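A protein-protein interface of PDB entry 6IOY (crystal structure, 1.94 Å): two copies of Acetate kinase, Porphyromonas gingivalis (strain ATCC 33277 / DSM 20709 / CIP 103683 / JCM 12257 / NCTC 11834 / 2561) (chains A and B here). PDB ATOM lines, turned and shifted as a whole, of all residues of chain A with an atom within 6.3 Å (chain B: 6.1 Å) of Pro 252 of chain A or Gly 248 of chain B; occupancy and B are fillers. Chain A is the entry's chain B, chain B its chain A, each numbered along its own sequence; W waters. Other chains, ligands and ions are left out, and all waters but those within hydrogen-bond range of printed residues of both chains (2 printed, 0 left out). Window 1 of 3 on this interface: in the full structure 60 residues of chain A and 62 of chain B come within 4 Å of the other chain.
Printed residues of chain B within 4 Å of Ala 168 of chain A: Met 242 (3.7 Å), Ser 247 (3.4 Å) and Gly 278 (3.0 Å).
Pro 252 of chain A touches just these residues of chain B: Val 238, Gly 248, Val 250, Leu 255 and Ile 273.
Of the printed residues of chain B, Gly 253 of chain A touches Thr 236 and Val 238.
Of chain A, only Pro 252 comes within 4 Å of Gly 248 of chain B.
Asp 249 of chain B touches none of the printed residues of chain A.
Of the printed residues of chain A, Val 250 of chain B touches Pro 252 (3.5 Å).
The nearest residue of chain B that does not touch Pro 252 of chain A is Glu 239 of chain B (4.1 Å).
The nearest residue of chain A that does not touch Gly 248 of chain B is Ala 168 of chain A (5.5 Å).
Among the printed residues, pairs that only touch across the chains: Asp 251 of chain A with Glu 239 of chain B, Gly 253 of chain A with Val 238 of chain B, Ala 168 of chain A with Ser 247 of chain B, Asp 251 of chain A with Val 238 of chain B, Gly 253 of chain A with Thr 236 of chain B, Pro 252 of chain A with Val 250 of chain B, Pro 252 of chain A with Leu 255 of chain B, Pro 252 of chain A with Ile 273 of chain B, Pro 252 of chain A with Gly 248 of chain B, Ala 168 of chain A with Met 242 of chain B and Pro 252 of chain A with Val 238 of chain B.
The backbone NH (N) of Thr 236 of chain B sits at hydrogen-bond distance from the side-chain carboxylate (OD2) of Asp 251 of chain A (2.8 Å).
O of Ala 168 of chain A sits at hydrogen-bond distance from N of Gly 278 of chain B.
Hydrophobic or aromatic side chains of chain A within 4 Å of the printed part of chain B: Ala 168 and Pro 252.
Along chain A the printed residues that touch a printed residue of chain B span positions 168 to 253.
Printed residues of chain B that touch a printed residue of chain A: Thr 236, Val 238, Glu 239, Met 242, Ser 247, Gly 248, Val 250, Leu 255, Ile 273 and Gly 278.
Among the printed residues, 13 pairs touch across the chains.
Among the printed residues, no Asp or Glu carboxylate lies within 4 Å of a Lys or Arg side-chain nitrogen of the other chain.
Positions printed for both chains: 250 and 255.
Water W1 lies within hydrogen-bond range of O of Val 250 of chain B (2.8 Å) and O of Val 250 of chain A (3.0 Å).
Water W2 bridges the backbone carbonyl oxygen (O) of Val 250 of chain A and the backbone NH (N) of Val 250 of chain B.
N of Val 238 of chain B lies close to OG1 of Thr 236 of chain B, 3.3 Å away.
The backbone NH of Gly 248 of chain B sits close to the backbone carbonyl oxygen of Val 238 of chain B (3.0 Å).
The backbone NH (N) of Gly 278 of chain B lies close to the backbone carbonyl oxygen (O) of Arg 246 of chain B, at 3.4 Å.
The backbone NH (N) of Ser 247 of chain B is in hydrogen-bond range of the backbone carbonyl oxygen (O) of Ile 273 of chain B (3.0 Å).
The side-chain carboxylate (OD1) of Asp 251 of chain A sits at hydrogen-bond distance from the backbone NH (N) of Gly 253 of chain A (2.9 Å).
The side-chain hydroxyl (OG1) of Thr 256 of chain A is in hydrogen-bond range of the backbone carbonyl oxygen (O) of Gly 253 of chain A, at 3.2 Å.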
ATOM      1  N   ALA A 168     -33.927  -8.567  -0.853  1.00  0.00           N
ATOM      2  CA  ALA A 168     -33.015  -8.300   0.238  1.00  0.00           C
ATOM      3  C   ALA A 168     -32.525  -6.847   0.122  1.00  0.00           C
ATOM      4  O   ALA A 168     -31.337  -6.572   0.008  1.00  0.00           O
ATOM      5  CB  ALA A 168     -31.872  -9.294   0.195  1.00  0.00           C
ATOM      6  N   VAL A 250     -29.433  -9.960 -14.171  1.00  0.00           N
ATOM      7  CA  VAL A 250     -28.104  -9.450 -14.349  1.00  0.00           C
ATOM      8  C   VAL A 250     -27.584  -8.882 -13.024  1.00  0.00           C
ATOM      9  O   VAL A 250     -28.350  -8.466 -12.171  1.00  0.00           O
ATOM     10  CB  VAL A 250     -28.069  -8.368 -15.447  1.00  0.00           C
ATOM     11  CG1 VAL A 250     -28.558  -8.940 -16.774  1.00  0.00           C
ATOM     12  CG2 VAL A 250     -28.872  -7.146 -15.060  1.00  0.00           C
ATOM     13  N   ASP A 251     -26.254  -8.759 -12.941  1.00  0.00           N
ATOM     14  CA  ASP A 251     -25.560  -8.222 -11.787  1.00  0.00           C
ATOM     15  C   ASP A 251     -26.066  -6.806 -11.524  1.00  0.00           C
ATOM     16  O   ASP A 251     -25.928  -5.945 -12.391  1.00  0.00           O
ATOM     17  CB  ASP A 251     -24.047  -8.277 -12.062  1.00  0.00           C
ATOM     18  CG  ASP A 251     -23.113  -7.671 -11.013  1.00  0.00           C
ATOM     19  OD1 ASP A 251     -23.612  -7.131 -10.035  1.00  0.00           O
ATOM     20  OD2 ASP A 251     -21.904  -7.768 -11.197  1.00  0.00           O
ATOM     21  N   PRO A 252     -26.655  -6.503 -10.342  1.00  0.00           N
ATOM     22  CA  PRO A 252     -27.135  -5.152 -10.053  1.00  0.00           C
ATOM     23  C   PRO A 252     -26.030  -4.093 -10.208  1.00  0.00           C
ATOM     24  O   PRO A 252     -26.282  -2.954 -10.627  1.00  0.00           O
ATOM     25  CB  PRO A 252     -27.580  -5.215  -8.587  1.00  0.00           C
ATOM     26  CG  PRO A 252     -27.787  -6.679  -8.287  1.00  0.00           C
ATOM     27  CD  PRO A 252     -26.861  -7.428  -9.218  1.00  0.00           C
ATOM     28  N   GLY A 253     -24.800  -4.495  -9.890  1.00  0.00           N
ATOM     29  CA  GLY A 253     -23.633  -3.639 -10.006  1.00  0.00           C
ATOM     30  C   GLY A 253     -23.228  -3.346 -11.441  1.00  0.00           C
ATOM     31  O   GLY A 253     -22.519  -2.357 -11.683  1.00  0.00           O
ATOM     32  N   VAL A 254     -23.586  -4.216 -12.393  1.00  0.00           N
ATOM     33  CA  VAL A 254     -23.343  -3.944 -13.809  1.00  0.00           C
ATOM     34  C   VAL A 254     -24.229  -2.759 -14.236  1.00  0.00           C
ATOM     35  O   VAL A 254     -23.812  -1.919 -15.017  1.00  0.00           O
ATOM     36  CB  VAL A 254     -23.577  -5.180 -14.691  1.00  0.00           C
ATOM     37  CG1 VAL A 254     -23.799  -4.827 -16.148  1.00  0.00           C
ATOM     38  CG2 VAL A 254     -22.438  -6.165 -14.582  1.00  0.00           C
ATOM     39  N   LEU A 255     -25.452  -2.698 -13.719  1.00  0.00           N
ATOM     40  CA  LEU A 255     -26.386  -1.648 -14.110  1.00  0.00           C
ATOM     41  C   LEU A 255     -25.848  -0.286 -13.643  1.00  0.00           C
ATOM     42  O   LEU A 255     -25.825   0.660 -14.430  1.00  0.00           O
ATOM     43  CB  LEU A 255     -27.773  -1.896 -13.515  1.00  0.00           C
ATOM     44  CG  LEU A 255     -28.658  -2.974 -14.155  1.00  0.00           C
ATOM     45  CD1 LEU A 255     -30.104  -2.503 -14.134  1.00  0.00           C
ATOM     46  CD2 LEU A 255     -28.271  -3.318 -15.589  1.00  0.00           C
ATOM     47  N   THR A 256     -25.408  -0.184 -12.381  1.00  0.00           N
ATOM     48  CA  THR A 256     -24.850   1.076 -11.883  1.00  0.00           C
ATOM     49  C   THR A 256     -23.541   1.412 -12.618  1.00  0.00           C
ATOM     50  O   THR A 256     -23.248   2.582 -12.911  1.00  0.00           O
ATOM     51  CB  THR A 256     -24.705   1.055 -10.355  1.00  0.00           C
ATOM     52  OG1 THR A 256     -23.831   0.023  -9.942  1.00  0.00           O
ATOM     53  CG2 THR A 256     -26.011   0.807  -9.642  1.00  0.00           C
ATOM     54  N   PHE A 257     -22.754   0.387 -12.955  1.00  0.00           N
ATOM     55  CA  PHE A 257     -21.540   0.597 -13.701  1.00  0.00           C
ATOM     56  C   PHE A 257     -21.862   1.208 -15.073  1.00  0.00           C
ATOM     57  O   PHE A 257     -21.184   2.153 -15.484  1.00  0.00           O
ATOM     58  CB  PHE A 257     -20.722  -0.692 -13.804  1.00  0.00           C
ATOM     59  CG  PHE A 257     -19.555  -0.590 -14.755  1.00  0.00           C
ATOM     60  CD1 PHE A 257     -18.350  -0.034 -14.353  1.00  0.00           C
ATOM     61  CD2 PHE A 257     -19.668  -1.032 -16.059  1.00  0.00           C
ATOM     62  CE1 PHE A 257     -17.294   0.089 -15.245  1.00  0.00           C
ATOM     63  CE2 PHE A 257     -18.594  -0.968 -16.933  1.00  0.00           C
ATOM     64  CZ  PHE A 257     -17.412  -0.393 -16.529  1.00  0.00           C
ATOM     65  N   THR B 236     -19.283  -7.445 -10.321  1.00  0.00           N
ATOM     66  CA  THR B 236     -19.207  -6.777  -9.043  1.00  0.00           C
ATOM     67  C   THR B 236     -19.605  -7.765  -7.962  1.00  0.00           C
ATOM     68  O   THR B 236     -20.323  -8.733  -8.238  1.00  0.00           O
ATOM     69  CB  THR B 236     -20.114  -5.536  -8.965  1.00  0.00           C
ATOM     70  OG1 THR B 236     -21.420  -5.932  -8.548  1.00  0.00           O
ATOM     71  CG2 THR B 236     -20.215  -4.791 -10.278  1.00  0.00           C
ATOM     72  N   VAL B 238     -21.869  -7.554  -5.701  1.00  0.00           N
ATOM     73  CA  VAL B 238     -23.230  -7.437  -5.171  1.00  0.00           C
ATOM     74  C   VAL B 238     -24.106  -8.620  -5.620  1.00  0.00           C
ATOM     75  O   VAL B 238     -25.060  -8.938  -4.919  1.00  0.00           O
ATOM     76  CB  VAL B 238     -23.882  -6.079  -5.479  1.00  0.00           C
ATOM     77  CG1 VAL B 238     -24.232  -5.916  -6.915  1.00  0.00           C
ATOM     78  CG2 VAL B 238     -25.118  -5.882  -4.645  1.00  0.00           C
ATOM     79  N   GLU B 239     -23.743  -9.293  -6.723  1.00  0.00           N
ATOM     80  CA  GLU B 239     -24.562 -10.303  -7.349  1.00  0.00           C
ATOM     81  C   GLU B 239     -24.528 -11.603  -6.529  1.00  0.00           C
ATOM     82  O   GLU B 239     -23.518 -11.919  -5.865  1.00  0.00           O
ATOM     83  CB  GLU B 239     -24.105 -10.571  -8.790  1.00  0.00           C
ATOM     84  CG  GLU B 239     -25.130 -11.403  -9.584  1.00  0.00           C
ATOM     85  CD  GLU B 239     -24.790 -11.724 -11.032  1.00  0.00           C
ATOM     86  OE1 GLU B 239     -23.661 -11.434 -11.480  1.00  0.00           O
ATOM     87  OE2 GLU B 239     -25.662 -12.317 -11.700  1.00  0.00           O
ATOM     88  N   GLY B 240     -25.648 -12.326  -6.608  1.00  0.00           N
ATOM     89  CA  GLY B 240     -25.733 -13.699  -6.194  1.00  0.00           C
ATOM     90  C   GLY B 240     -26.453 -13.849  -4.870  1.00  0.00           C
ATOM     91  O   GLY B 240     -27.656 -13.535  -4.728  1.00  0.00           O
ATOM     92  N   LEU B 241     -25.731 -14.392  -3.884  1.00  0.00           N
ATOM     93  CA  LEU B 241     -26.318 -14.722  -2.599  1.00  0.00           C
ATOM     94  C   LEU B 241     -26.593 -13.429  -1.827  1.00  0.00           C
ATOM     95  O   LEU B 241     -25.952 -12.406  -2.009  1.00  0.00           O
ATOM     96  CB  LEU B 241     -25.378 -15.608  -1.785  1.00  0.00           C
ATOM     97  CG  LEU B 241     -25.057 -16.966  -2.401  1.00  0.00           C
ATOM     98  CD1 LEU B 241     -24.015 -17.696  -1.569  1.00  0.00           C
ATOM     99  CD2 LEU B 241     -26.335 -17.772  -2.520  1.00  0.00           C
ATOM    100  N   MET B 242     -27.561 -13.532  -0.934  1.00  0.00           N
ATOM    101  CA  MET B 242     -27.789 -12.530   0.085  1.00  0.00           C
ATOM    102  C   MET B 242     -26.557 -12.480   1.002  1.00  0.00           C
ATOM    103  O   MET B 242     -25.961 -13.501   1.315  1.00  0.00           O
ATOM    104  CB  MET B 242     -29.048 -12.951   0.830  1.00  0.00           C
ATOM    105  CG  MET B 242     -29.630 -11.893   1.652  1.00  0.00           C
ATOM    106  SD  MET B 242     -31.221 -12.543   2.287  1.00  0.00           S
ATOM    107  CE  MET B 242     -31.483 -11.451   3.687  1.00  0.00           C
ATOM    108  N   MET B 243     -26.117 -11.271   1.359  1.00  0.00           N
ATOM    109  CA  MET B 243     -24.912 -11.099   2.166  1.00  0.00           C
ATOM    110  C   MET B 243     -25.209 -10.191   3.374  1.00  0.00           C
ATOM    111  O   MET B 243     -26.388  -9.836   3.608  1.00  0.00           O
ATOM    112  CB  MET B 243     -23.807 -10.498   1.312  1.00  0.00           C
ATOM    113  CG  MET B 243     -23.614 -11.212   0.013  1.00  0.00           C
ATOM    114  SD  MET B 243     -22.276 -10.575  -0.973  1.00  0.00           S
ATOM    115  CE  MET B 243     -22.839 -11.026  -2.619  1.00  0.00           C
ATOM    116  N   ARG B 246     -25.038  -6.538   1.423  1.00  0.00           N
ATOM    117  CA  ARG B 246     -25.259  -6.519  -0.009  1.00  0.00           C
ATOM    118  C   ARG B 246     -26.512  -7.332  -0.336  1.00  0.00           C
ATOM    119  O   ARG B 246     -26.823  -8.349   0.316  1.00  0.00           O
ATOM    120  CB  ARG B 246     -24.039  -7.069  -0.756  1.00  0.00           C
ATOM    121  CG  ARG B 246     -22.762  -6.267  -0.576  1.00  0.00           C
ATOM    122  CD  ARG B 246     -21.698  -6.726  -1.555  1.00  0.00           C
ATOM    123  NE  ARG B 246     -20.358  -6.333  -1.143  1.00  0.00           N
ATOM    124  CZ  ARG B 246     -19.396  -7.177  -0.762  1.00  0.00           C
ATOM    125  NH1 ARG B 246     -19.527  -8.470  -0.981  1.00  0.00           N
ATOM    126  NH2 ARG B 246     -18.309  -6.719  -0.164  1.00  0.00           N
ATOM    127  N   SER B 247     -27.207  -6.874  -1.369  1.00  0.00           N
ATOM    128  CA  SER B 247     -28.523  -7.376  -1.760  1.00  0.00           C
ATOM    129  C   SER B 247     -28.454  -8.801  -2.299  1.00  0.00           C
ATOM    130  O   SER B 247     -29.380  -9.553  -2.108  1.00  0.00           O
ATOM    131  CB  SER B 247     -29.157  -6.473  -2.782  1.00  0.00           C
ATOM    132  OG  SER B 247     -28.418  -6.451  -3.983  1.00  0.00           O
ATOM    133  N   GLY B 248     -27.379  -9.129  -3.017  1.00  0.00           N
ATOM    134  CA  GLY B 248     -27.415 -10.245  -3.931  1.00  0.00           C
ATOM    135  C   GLY B 248     -28.348  -9.946  -5.084  1.00  0.00           C
ATOM    136  O   GLY B 248     -28.626  -8.773  -5.374  1.00  0.00           O
ATOM    137  N   ASP B 249     -28.827 -11.026  -5.737  1.00  0.00           N
ATOM    138  CA  ASP B 249     -29.705 -10.975  -6.896  1.00  0.00           C
ATOM    139  C   ASP B 249     -30.949 -10.154  -6.562  1.00  0.00           C
ATOM    140  O   ASP B 249     -31.593 -10.373  -5.562  1.00  0.00           O
ATOM    141  CB  ASP B 249     -30.152 -12.367  -7.347  1.00  0.00           C
ATOM    142  CG  ASP B 249     -29.025 -13.284  -7.817  1.00  0.00           C
ATOM    143  OD1 ASP B 249     -27.971 -12.752  -8.249  1.00  0.00           O
ATOM    144  OD2 ASP B 249     -29.196 -14.534  -7.713  1.00  0.00           O
ATOM    145  N   VAL B 250     -31.253  -9.202  -7.447  1.00  0.00           N
ATOM    146  CA  VAL B 250     -32.466  -8.425  -7.376  1.00  0.00           C
ATOM    147  C   VAL B 250     -32.928  -8.131  -8.801  1.00  0.00           C
ATOM    148  O   VAL B 250     -32.148  -8.046  -9.731  1.00  0.00           O
ATOM    149  CB  VAL B 250     -32.267  -7.116  -6.582  1.00  0.00           C
ATOM    150  CG1 VAL B 250     -31.110  -6.335  -7.123  1.00  0.00           C
ATOM    151  CG2 VAL B 250     -33.519  -6.266  -6.591  1.00  0.00           C
ATOM    152  N   LEU B 255     -34.401  -1.839  -9.418  1.00  0.00           N
ATOM    153  CA  LEU B 255     -33.356  -0.843  -9.226  1.00  0.00           C
ATOM    154  C   LEU B 255     -33.742   0.462  -9.935  1.00  0.00           C
ATOM    155  O   LEU B 255     -33.687   1.520  -9.315  1.00  0.00           O
ATOM    156  CB  LEU B 255     -32.014  -1.350  -9.746  1.00  0.00           C
ATOM    157  CG  LEU B 255     -31.455  -2.568  -9.023  1.00  0.00           C
ATOM    158  CD1 LEU B 255     -29.998  -2.720  -9.386  1.00  0.00           C
ATOM    159  CD2 LEU B 255     -31.627  -2.437  -7.520  1.00  0.00           C
ATOM    160  N   ILE B 273     -27.493  -0.833  -2.436  1.00  0.00           N
ATOM    161  CA  ILE B 273     -27.420  -2.301  -2.647  1.00  0.00           C
ATOM    162  C   ILE B 273     -26.141  -2.898  -2.017  1.00  0.00           C
ATOM    163  O   ILE B 273     -26.086  -4.109  -1.754  1.00  0.00           O
ATOM    164  CB  ILE B 273     -27.547  -2.655  -4.135  1.00  0.00           C
ATOM    165  CG1 ILE B 273     -26.381  -2.114  -4.961  1.00  0.00           C
ATOM    166  CG2 ILE B 273     -28.888  -2.187  -4.669  1.00  0.00           C
ATOM    167  CD1 ILE B 273     -26.348  -2.573  -6.405  1.00  0.00           C
ATOM    168  N   GLY B 278     -29.234  -6.683   2.080  1.00  0.00           N
ATOM    169  CA  GLY B 278     -28.900  -7.983   2.637  1.00  0.00           C
ATOM    170  C   GLY B 278     -29.515  -8.203   4.007  1.00  0.00           C
ATOM    171  O   GLY B 278     -30.598  -7.760   4.294  1.00  0.00           O
HETATM  172  O   HOH W   1     -30.339  -6.474 -11.208  1.00  0.00           O
HETATM  173  O   HOH W   2     -29.486 -10.081 -10.137  1.00  0.00           O
